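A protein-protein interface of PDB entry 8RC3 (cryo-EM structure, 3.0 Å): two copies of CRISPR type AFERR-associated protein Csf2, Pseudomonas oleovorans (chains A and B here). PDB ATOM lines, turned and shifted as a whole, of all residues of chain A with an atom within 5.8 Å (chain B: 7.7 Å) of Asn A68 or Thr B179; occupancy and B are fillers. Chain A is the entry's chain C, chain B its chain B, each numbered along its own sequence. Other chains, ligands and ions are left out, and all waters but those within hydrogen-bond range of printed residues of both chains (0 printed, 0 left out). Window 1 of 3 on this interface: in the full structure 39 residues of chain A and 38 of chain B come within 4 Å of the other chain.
The guanidinium group of Arg A44 sits at hydrogen-bond distance from the backbone carbonyl oxygen of Trp B178 (3.0 Å).
The backbone NH (N) of Val A146 sits at hydrogen-bond distance from the backbone carbonyl oxygen (O) of Ala B289 (3.1 Å).
The backbone carbonyl oxygen of Val A146 lies close to the backbone carbonyl oxygen of Lys B290.
No position is printed for both chains.
Of the 6 pairs that touch across the chains among the printed residues, none has its exchanged pair printed and touching as well.
Asn A68 touches just these residues of chain B: Thr B179 (3.3 Å) and Arg B180 (3.6 Å).
Thr B179 touches just one residue of chain A: Asn A68 (3.3 Å).
No residue of chain B comes within 4 Å of Gly A67.
Printed residues of chain B within 4 Å of Val A146: Ala B289 (3.1 Å) and Lys B290 (3.2 Å).
Printed residues of chain A within 4 Å of Lys B290: Val A146 (3.2 Å).
Of the printed residues of chain B, Arg A71 touches Ala B289.
Of the printed residues of chain B, Arg A44 touches Trp B178.
The nearest residue of chain B that does not touch Asn A68 is Lys B290 (4.3 Å).
The nearest printed residue of chain A that does not touch Lys B290 is Asn A68 (4.3 Å).
The backbone NH (N) of Thr B179 sits at hydrogen-bond distance from the backbone carbonyl oxygen (O) of Asn B244 (2.7 Å).
The side-chain hydroxyl of Thr B179 sits close to a ring nitrogen (ND1) of His B246, at 3.4 Å.
Of the 15 printed residues of chain B, 5 touch a printed residue of chain A.
Hydrophobic or aromatic side chains of chain B within 4 Å of the printed part of chain A: Trp B178 and Ala B289.
Of the 10 printed residues of chain A, 4 touch a printed residue of chain B.
Printed residues of chain A that touch a printed residue of chain B: Arg A44, Asn A68, Arg A71 and Val A146.
Among the printed residues, 6 pairs touch across the chains.
Among the printed residues, no Asp or Glu carboxylate lies within 4 Å of a Lys or Arg side-chain nitrogen of the other chain.
Among the printed residues, merely in contact across the chains: Asn A68 with Thr B179 (3.3 Å), Asn A68 with Arg B180 (3.6 Å) and Arg A71 with Ala B289 (3.6 Å).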
ATOM      1  N   ARG A  44      16.402   3.925 -18.813  1.00  0.00           N
ATOM      2  CA  ARG A  44      15.978   2.535 -18.888  1.00  0.00           C
ATOM      3  C   ARG A  44      15.570   2.181 -20.309  1.00  0.00           C
ATOM      4  O   ARG A  44      14.821   2.918 -20.956  1.00  0.00           O
ATOM      5  CB  ARG A  44      14.824   2.273 -17.929  1.00  0.00           C
ATOM      6  CG  ARG A  44      14.513   0.806 -17.779  1.00  0.00           C
ATOM      7  CD  ARG A  44      13.286   0.593 -16.938  1.00  0.00           C
ATOM      8  NE  ARG A  44      13.547   0.816 -15.523  1.00  0.00           N
ATOM      9  CZ  ARG A  44      13.315  -0.077 -14.571  1.00  0.00           C
ATOM     10  NH1 ARG A  44      12.795  -1.261 -14.848  1.00  0.00           N
ATOM     11  NH2 ARG A  44      13.607   0.228 -13.311  1.00  0.00           N
ATOM     12  N   PRO A  66       8.905   2.381 -17.724  1.00  0.00           N
ATOM     13  CA  PRO A  66       8.331   1.084 -17.352  1.00  0.00           C
ATOM     14  C   PRO A  66       6.832   1.171 -17.118  1.00  0.00           C
ATOM     15  O   PRO A  66       6.301   2.206 -16.709  1.00  0.00           O
ATOM     16  CB  PRO A  66       9.069   0.717 -16.060  1.00  0.00           C
ATOM     17  CG  PRO A  66      10.182   1.668 -15.939  1.00  0.00           C
ATOM     18  CD  PRO A  66       9.854   2.879 -16.720  1.00  0.00           C
ATOM     19  N   GLY A  67       6.149   0.060 -17.389  1.00  0.00           N
ATOM     20  CA  GLY A  67       4.712   0.016 -17.195  1.00  0.00           C
ATOM     21  C   GLY A  67       4.302   0.229 -15.754  1.00  0.00           C
ATOM     22  O   GLY A  67       3.240   0.796 -15.487  1.00  0.00           O
ATOM     23  N   ASN A  68       5.126  -0.224 -14.810  1.00  0.00           N
ATOM     24  CA  ASN A  68       4.834   0.016 -13.401  1.00  0.00           C
ATOM     25  C   ASN A  68       4.855   1.504 -13.082  1.00  0.00           C
ATOM     26  O   ASN A  68       4.019   1.995 -12.314  1.00  0.00           O
ATOM     27  CB  ASN A  68       5.833  -0.734 -12.524  1.00  0.00           C
ATOM     28  CG  ASN A  68       5.257  -1.101 -11.179  1.00  0.00           C
ATOM     29  OD1 ASN A  68       4.059  -0.953 -10.948  1.00  0.00           O
ATOM     30  ND2 ASN A  68       6.104  -1.579 -10.281  1.00  0.00           N
ATOM     31  N   THR A  69       5.805   2.239 -13.664  1.00  0.00           N
ATOM     32  CA  THR A  69       5.889   3.676 -13.433  1.00  0.00           C
ATOM     33  C   THR A  69       4.626   4.383 -13.910  1.00  0.00           C
ATOM     34  O   THR A  69       4.049   5.200 -13.187  1.00  0.00           O
ATOM     35  CB  THR A  69       7.118   4.248 -14.135  1.00  0.00           C
ATOM     36  OG1 THR A  69       8.306   3.771 -13.494  1.00  0.00           O
ATOM     37  CG2 THR A  69       7.100   5.758 -14.085  1.00  0.00           C
ATOM     38  N   MET A  70       4.171   4.064 -15.124  1.00  0.00           N
ATOM     39  CA  MET A  70       2.967   4.700 -15.647  1.00  0.00           C
ATOM     40  C   MET A  70       1.720   4.258 -14.894  1.00  0.00           C
ATOM     41  O   MET A  70       0.793   5.054 -14.714  1.00  0.00           O
ATOM     42  CB  MET A  70       2.822   4.407 -17.137  1.00  0.00           C
ATOM     43  CG  MET A  70       4.101   4.558 -17.925  1.00  0.00           C
ATOM     44  SD  MET A  70       4.525   6.267 -18.287  1.00  0.00           S
ATOM     45  CE  MET A  70       2.923   6.947 -18.679  1.00  0.00           C
ATOM     46  N   ARG A  71       1.673   2.999 -14.455  1.00  0.00           N
ATOM     47  CA  ARG A  71       0.536   2.535 -13.666  1.00  0.00           C
ATOM     48  C   ARG A  71       0.442   3.287 -12.348  1.00  0.00           C
ATOM     49  O   ARG A  71      -0.646   3.705 -11.936  1.00  0.00           O
ATOM     50  CB  ARG A  71       0.649   1.033 -13.421  1.00  0.00           C
ATOM     51  CG  ARG A  71      -0.557   0.422 -12.746  1.00  0.00           C
ATOM     52  CD  ARG A  71      -0.476  -1.088 -12.747  1.00  0.00           C
ATOM     53  NE  ARG A  71      -1.356  -1.679 -11.749  1.00  0.00           N
ATOM     54  CZ  ARG A  71      -2.481  -2.319 -12.027  1.00  0.00           C
ATOM     55  NH1 ARG A  71      -2.896  -2.480 -13.271  1.00  0.00           N
ATOM     56  NH2 ARG A  71      -3.209  -2.811 -11.030  1.00  0.00           N
ATOM     57  N   ASN A  72       1.577   3.483 -11.677  1.00  0.00           N
ATOM     58  CA  ASN A  72       1.558   4.262 -10.446  1.00  0.00           C
ATOM     59  C   ASN A  72       1.266   5.728 -10.719  1.00  0.00           C
ATOM     60  O   ASN A  72       0.651   6.395  -9.884  1.00  0.00           O
ATOM     61  CB  ASN A  72       2.877   4.123  -9.700  1.00  0.00           C
ATOM     62  CG  ASN A  72       2.837   4.776  -8.343  1.00  0.00           C
ATOM     63  OD1 ASN A  72       3.157   5.953  -8.199  1.00  0.00           O
ATOM     64  ND2 ASN A  72       2.431   4.017  -7.336  1.00  0.00           N
ATOM     65  N   LEU A  73       1.700   6.249 -11.866  1.00  0.00           N
ATOM     66  CA  LEU A  73       1.348   7.615 -12.237  1.00  0.00           C
ATOM     67  C   LEU A  73      -0.160   7.767 -12.369  1.00  0.00           C
ATOM     68  O   LEU A  73      -0.747   8.729 -11.863  1.00  0.00           O
ATOM     69  CB  LEU A  73       2.045   7.995 -13.542  1.00  0.00           C
ATOM     70  CG  LEU A  73       1.580   9.276 -14.228  1.00  0.00           C
ATOM     71  CD1 LEU A  73       2.021  10.488 -13.438  1.00  0.00           C
ATOM     72  CD2 LEU A  73       2.115   9.339 -15.640  1.00  0.00           C
ATOM     73  N   VAL A 146      -1.832  -1.740 -17.513  1.00  0.00           N
ATOM     74  CA  VAL A 146      -1.063  -0.580 -17.942  1.00  0.00           C
ATOM     75  C   VAL A 146       0.229  -1.059 -18.582  1.00  0.00           C
ATOM     76  O   VAL A 146       0.989  -1.821 -17.972  1.00  0.00           O
ATOM     77  CB  VAL A 146      -0.774   0.366 -16.766  1.00  0.00           C
ATOM     78  CG1 VAL A 146       0.157   1.475 -17.207  1.00  0.00           C
ATOM     79  CG2 VAL A 146      -2.061   0.939 -16.221  1.00  0.00           C
ATOM     80  N   PRO B  39      16.015 -10.452  -5.267  1.00  0.00           N
ATOM     81  CA  PRO B  39      15.183 -11.564  -5.736  1.00  0.00           C
ATOM     82  C   PRO B  39      14.773 -11.376  -7.188  1.00  0.00           C
ATOM     83  O   PRO B  39      14.468 -10.268  -7.629  1.00  0.00           O
ATOM     84  CB  PRO B  39      13.976 -11.529  -4.793  1.00  0.00           C
ATOM     85  CG  PRO B  39      14.014 -10.195  -4.150  1.00  0.00           C
ATOM     86  CD  PRO B  39      15.442  -9.796  -4.084  1.00  0.00           C
ATOM     87  N   ILE B 176      15.437  -8.561 -18.454  1.00  0.00           N
ATOM     88  CA  ILE B 176      15.188  -8.436 -17.021  1.00  0.00           C
ATOM     89  C   ILE B 176      14.585  -7.066 -16.738  1.00  0.00           C
ATOM     90  O   ILE B 176      15.107  -6.041 -17.192  1.00  0.00           O
ATOM     91  CB  ILE B 176      16.473  -8.668 -16.206  1.00  0.00           C
ATOM     92  CG1 ILE B 176      16.179  -8.614 -14.710  1.00  0.00           C
ATOM     93  CG2 ILE B 176      17.570  -7.693 -16.599  1.00  0.00           C
ATOM     94  CD1 ILE B 176      17.318  -9.099 -13.859  1.00  0.00           C
ATOM     95  N   VAL B 177      13.478  -7.051 -15.999  1.00  0.00           N
ATOM     96  CA  VAL B 177      12.749  -5.831 -15.672  1.00  0.00           C
ATOM     97  C   VAL B 177      12.791  -5.631 -14.165  1.00  0.00           C
ATOM     98  O   VAL B 177      12.445  -6.540 -13.402  1.00  0.00           O
ATOM     99  CB  VAL B 177      11.298  -5.890 -16.175  1.00  0.00           C
ATOM    100  CG1 VAL B 177      10.480  -4.779 -15.552  1.00  0.00           C
ATOM    101  CG2 VAL B 177      11.260  -5.790 -17.682  1.00  0.00           C
ATOM    102  N   TRP B 178      13.206  -4.443 -13.738  1.00  0.00           N
ATOM    103  CA  TRP B 178      13.316  -4.131 -12.322  1.00  0.00           C
ATOM    104  C   TRP B 178      12.048  -3.449 -11.831  1.00  0.00           C
ATOM    105  O   TRP B 178      11.497  -2.575 -12.502  1.00  0.00           O
ATOM    106  CB  TRP B 178      14.530  -3.244 -12.060  1.00  0.00           C
ATOM    107  CG  TRP B 178      15.819  -3.984 -12.131  1.00  0.00           C
ATOM    108  CD1 TRP B 178      16.624  -4.117 -13.217  1.00  0.00           C
ATOM    109  CD2 TRP B 178      16.455  -4.698 -11.069  1.00  0.00           C
ATOM    110  NE1 TRP B 178      17.724  -4.872 -12.901  1.00  0.00           N
ATOM    111  CE2 TRP B 178      17.642  -5.241 -11.586  1.00  0.00           C
ATOM    112  CE3 TRP B 178      16.131  -4.939  -9.734  1.00  0.00           C
ATOM    113  CZ2 TRP B 178      18.506  -6.005 -10.815  1.00  0.00           C
ATOM    114  CZ3 TRP B 178      16.993  -5.698  -8.970  1.00  0.00           C
ATOM    115  CH2 TRP B 178      18.164  -6.220  -9.510  1.00  0.00           C
ATOM    116  N   THR B 179      11.591  -3.860 -10.653  1.00  0.00           N
ATOM    117  CA  THR B 179      10.327  -3.408 -10.094  1.00  0.00           C
ATOM    118  C   THR B 179      10.560  -2.876  -8.689  1.00  0.00           C
ATOM    119  O   THR B 179      11.354  -3.435  -7.928  1.00  0.00           O
ATOM    120  CB  THR B 179       9.301  -4.550 -10.076  1.00  0.00           C
ATOM    121  OG1 THR B 179       9.033  -4.972 -11.418  1.00  0.00           O
ATOM    122  CG2 THR B 179       8.001  -4.114  -9.426  1.00  0.00           C
ATOM    123  N   ARG B 180       9.863  -1.796  -8.352  1.00  0.00           N
ATOM    124  CA  ARG B 180      10.022  -1.118  -7.078  1.00  0.00           C
ATOM    125  C   ARG B 180       8.669  -0.973  -6.398  1.00  0.00           C
ATOM    126  O   ARG B 180       7.631  -0.922  -7.060  1.00  0.00           O
ATOM    127  CB  ARG B 180      10.659   0.259  -7.276  1.00  0.00           C
ATOM    128  CG  ARG B 180      10.991   0.989  -6.005  1.00  0.00           C
ATOM    129  CD  ARG B 180      12.064   2.015  -6.242  1.00  0.00           C
ATOM    130  NE  ARG B 180      11.520   3.310  -6.619  1.00  0.00           N
ATOM    131  CZ  ARG B 180      11.388   4.330  -5.784  1.00  0.00           C
ATOM    132  NH1 ARG B 180      11.733   4.228  -4.512  1.00  0.00           N
ATOM    133  NH2 ARG B 180      10.895   5.478  -6.237  1.00  0.00           N
ATOM    134  N   ARG B 181       8.685  -0.937  -5.068  1.00  0.00           N
ATOM    135  CA  ARG B 181       7.518  -0.573  -4.279  1.00  0.00           C
ATOM    136  C   ARG B 181       7.923   0.481  -3.263  1.00  0.00           C
ATOM    137  O   ARG B 181       9.011   0.416  -2.686  1.00  0.00           O
ATOM    138  CB  ARG B 181       6.900  -1.773  -3.564  1.00  0.00           C
ATOM    139  CG  ARG B 181       5.543  -1.468  -2.953  1.00  0.00           C
ATOM    140  CD  ARG B 181       4.767  -2.721  -2.626  1.00  0.00           C
ATOM    141  NE  ARG B 181       5.540  -3.645  -1.810  1.00  0.00           N
ATOM    142  CZ  ARG B 181       5.072  -4.789  -1.333  1.00  0.00           C
ATOM    143  NH1 ARG B 181       3.833  -5.182  -1.575  1.00  0.00           N
ATOM    144  NH2 ARG B 181       5.865  -5.555  -0.592  1.00  0.00           N
ATOM    145  N   ALA B 242      10.255  -2.265  -1.414  1.00  0.00           N
ATOM    146  CA  ALA B 242      10.693  -3.477  -2.083  1.00  0.00           C
ATOM    147  C   ALA B 242      11.391  -3.111  -3.381  1.00  0.00           C
ATOM    148  O   ALA B 242      10.942  -2.221  -4.106  1.00  0.00           O
ATOM    149  CB  ALA B 242       9.519  -4.416  -2.369  1.00  0.00           C
ATOM    150  N   PHE B 243      12.489  -3.805  -3.666  1.00  0.00           N
ATOM    151  CA  PHE B 243      13.188  -3.676  -4.940  1.00  0.00           C
ATOM    152  C   PHE B 243      13.586  -5.070  -5.394  1.00  0.00           C
ATOM    153  O   PHE B 243      14.477  -5.687  -4.803  1.00  0.00           O
ATOM    154  CB  PHE B 243      14.411  -2.774  -4.823  1.00  0.00           C
ATOM    155  CG  PHE B 243      14.971  -2.346  -6.145  1.00  0.00           C
ATOM    156  CD1 PHE B 243      14.195  -1.645  -7.044  1.00  0.00           C
ATOM    157  CD2 PHE B 243      16.267  -2.655  -6.491  1.00  0.00           C
ATOM    158  CE1 PHE B 243      14.699  -1.256  -8.254  1.00  0.00           C
ATOM    159  CE2 PHE B 243      16.777  -2.262  -7.705  1.00  0.00           C
ATOM    160  CZ  PHE B 243      15.992  -1.564  -8.587  1.00  0.00           C
ATOM    161  N   ASN B 244      12.931  -5.566  -6.438  1.00  0.00           N
ATOM    162  CA  ASN B 244      13.226  -6.874  -6.990  1.00  0.00           C
ATOM    163  C   ASN B 244      13.117  -6.795  -8.504  1.00  0.00           C
ATOM    164  O   ASN B 244      12.822  -5.742  -9.072  1.00  0.00           O
ATOM    165  CB  ASN B 244      12.287  -7.940  -6.420  1.00  0.00           C
ATOM    166  CG  ASN B 244      10.855  -7.477  -6.369  1.00  0.00           C
ATOM    167  OD1 ASN B 244      10.264  -7.142  -7.392  1.00  0.00           O
ATOM    168  ND2 ASN B 244      10.285  -7.452  -5.173  1.00  0.00           N
ATOM    169  N   ALA B 245      13.351  -7.926  -9.160  1.00  0.00           N
ATOM    170  CA  ALA B 245      13.305  -7.994 -10.609  1.00  0.00           C
ATOM    171  C   ALA B 245      12.555  -9.244 -11.032  1.00  0.00           C
ATOM    172  O   ALA B 245      12.433 -10.209 -10.275  1.00  0.00           O
ATOM    173  CB  ALA B 245      14.706  -7.994 -11.224  1.00  0.00           C
ATOM    174  N   HIS B 246      12.037  -9.207 -12.253  1.00  0.00           N
ATOM    175  CA  HIS B 246      11.481 -10.385 -12.891  1.00  0.00           C
ATOM    176  C   HIS B 246      11.977 -10.421 -14.326  1.00  0.00           C
ATOM    177  O   HIS B 246      12.286  -9.383 -14.915  1.00  0.00           O
ATOM    178  CB  HIS B 246       9.948 -10.398 -12.844  1.00  0.00           C
ATOM    179  CG  HIS B 246       9.311  -9.242 -13.545  1.00  0.00           C
ATOM    180  ND1 HIS B 246       9.075  -8.035 -12.927  1.00  0.00           N
ATOM    181  CD2 HIS B 246       8.851  -9.114 -14.811  1.00  0.00           C
ATOM    182  CE1 HIS B 246       8.505  -7.209 -13.786  1.00  0.00           C
ATOM    183  NE2 HIS B 246       8.357  -7.840 -14.936  1.00  0.00           N
ATOM    184  N   ALA B 289      -0.931  -6.789 -14.392  1.00  0.00           N
ATOM    185  CA  ALA B 289      -0.762  -5.372 -14.097  1.00  0.00           C
ATOM    186  C   ALA B 289       0.045  -4.670 -15.180  1.00  0.00           C
ATOM    187  O   ALA B 289      -0.279  -3.544 -15.573  1.00  0.00           O
ATOM    188  CB  ALA B 289      -0.092  -5.204 -12.738  1.00  0.00           C
ATOM    189  N   LYS B 290       1.091  -5.320 -15.680  1.00  0.00           N
ATOM    190  CA  LYS B 290       1.996  -4.725 -16.649  1.00  0.00           C
ATOM    191  C   LYS B 290       1.580  -4.982 -18.091  1.00  0.00           C
ATOM    192  O   LYS B 290       2.352  -4.679 -19.004  1.00  0.00           O
ATOM    193  CB  LYS B 290       3.416  -5.243 -16.425  1.00  0.00           C
ATOM    194  CG  LYS B 290       4.247  -4.400 -15.479  1.00  0.00           C
ATOM    195  CD  LYS B 290       3.976  -4.748 -14.031  1.00  0.00           C
ATOM    196  CE  LYS B 290       4.656  -6.045 -13.644  1.00  0.00           C
ATOM    197  NZ  LYS B 290       4.523  -6.309 -12.188  1.00  0.00           N
ATOM    198  N   TYR B 292       1.327  -7.757 -19.714  1.00  0.00           N
ATOM    199  CA  TYR B 292       2.144  -8.772 -20.356  1.00  0.00           C
ATOM    200  C   TYR B 292       1.264  -9.775 -21.094  1.00  0.00           C
ATOM    201  O   TYR B 292       0.054  -9.858 -20.878  1.00  0.00           O
ATOM    202  CB  TYR B 292       3.002  -9.508 -19.328  1.00  0.00           C
ATOM    203  CG  TYR B 292       4.124  -8.687 -18.742  1.00  0.00           C
ATOM    204  CD1 TYR B 292       4.657  -7.613 -19.425  1.00  0.00           C
ATOM    205  CD2 TYR B 292       4.643  -8.990 -17.496  1.00  0.00           C
ATOM    206  CE1 TYR B 292       5.677  -6.867 -18.885  1.00  0.00           C
ATOM    207  CE2 TYR B 292       5.662  -8.252 -16.952  1.00  0.00           C
ATOM    208  CZ  TYR B 292       6.176  -7.192 -17.649  1.00  0.00           C
ATOM    209  OH  TYR B 292       7.195  -6.454 -17.105  1.00  0.00           O
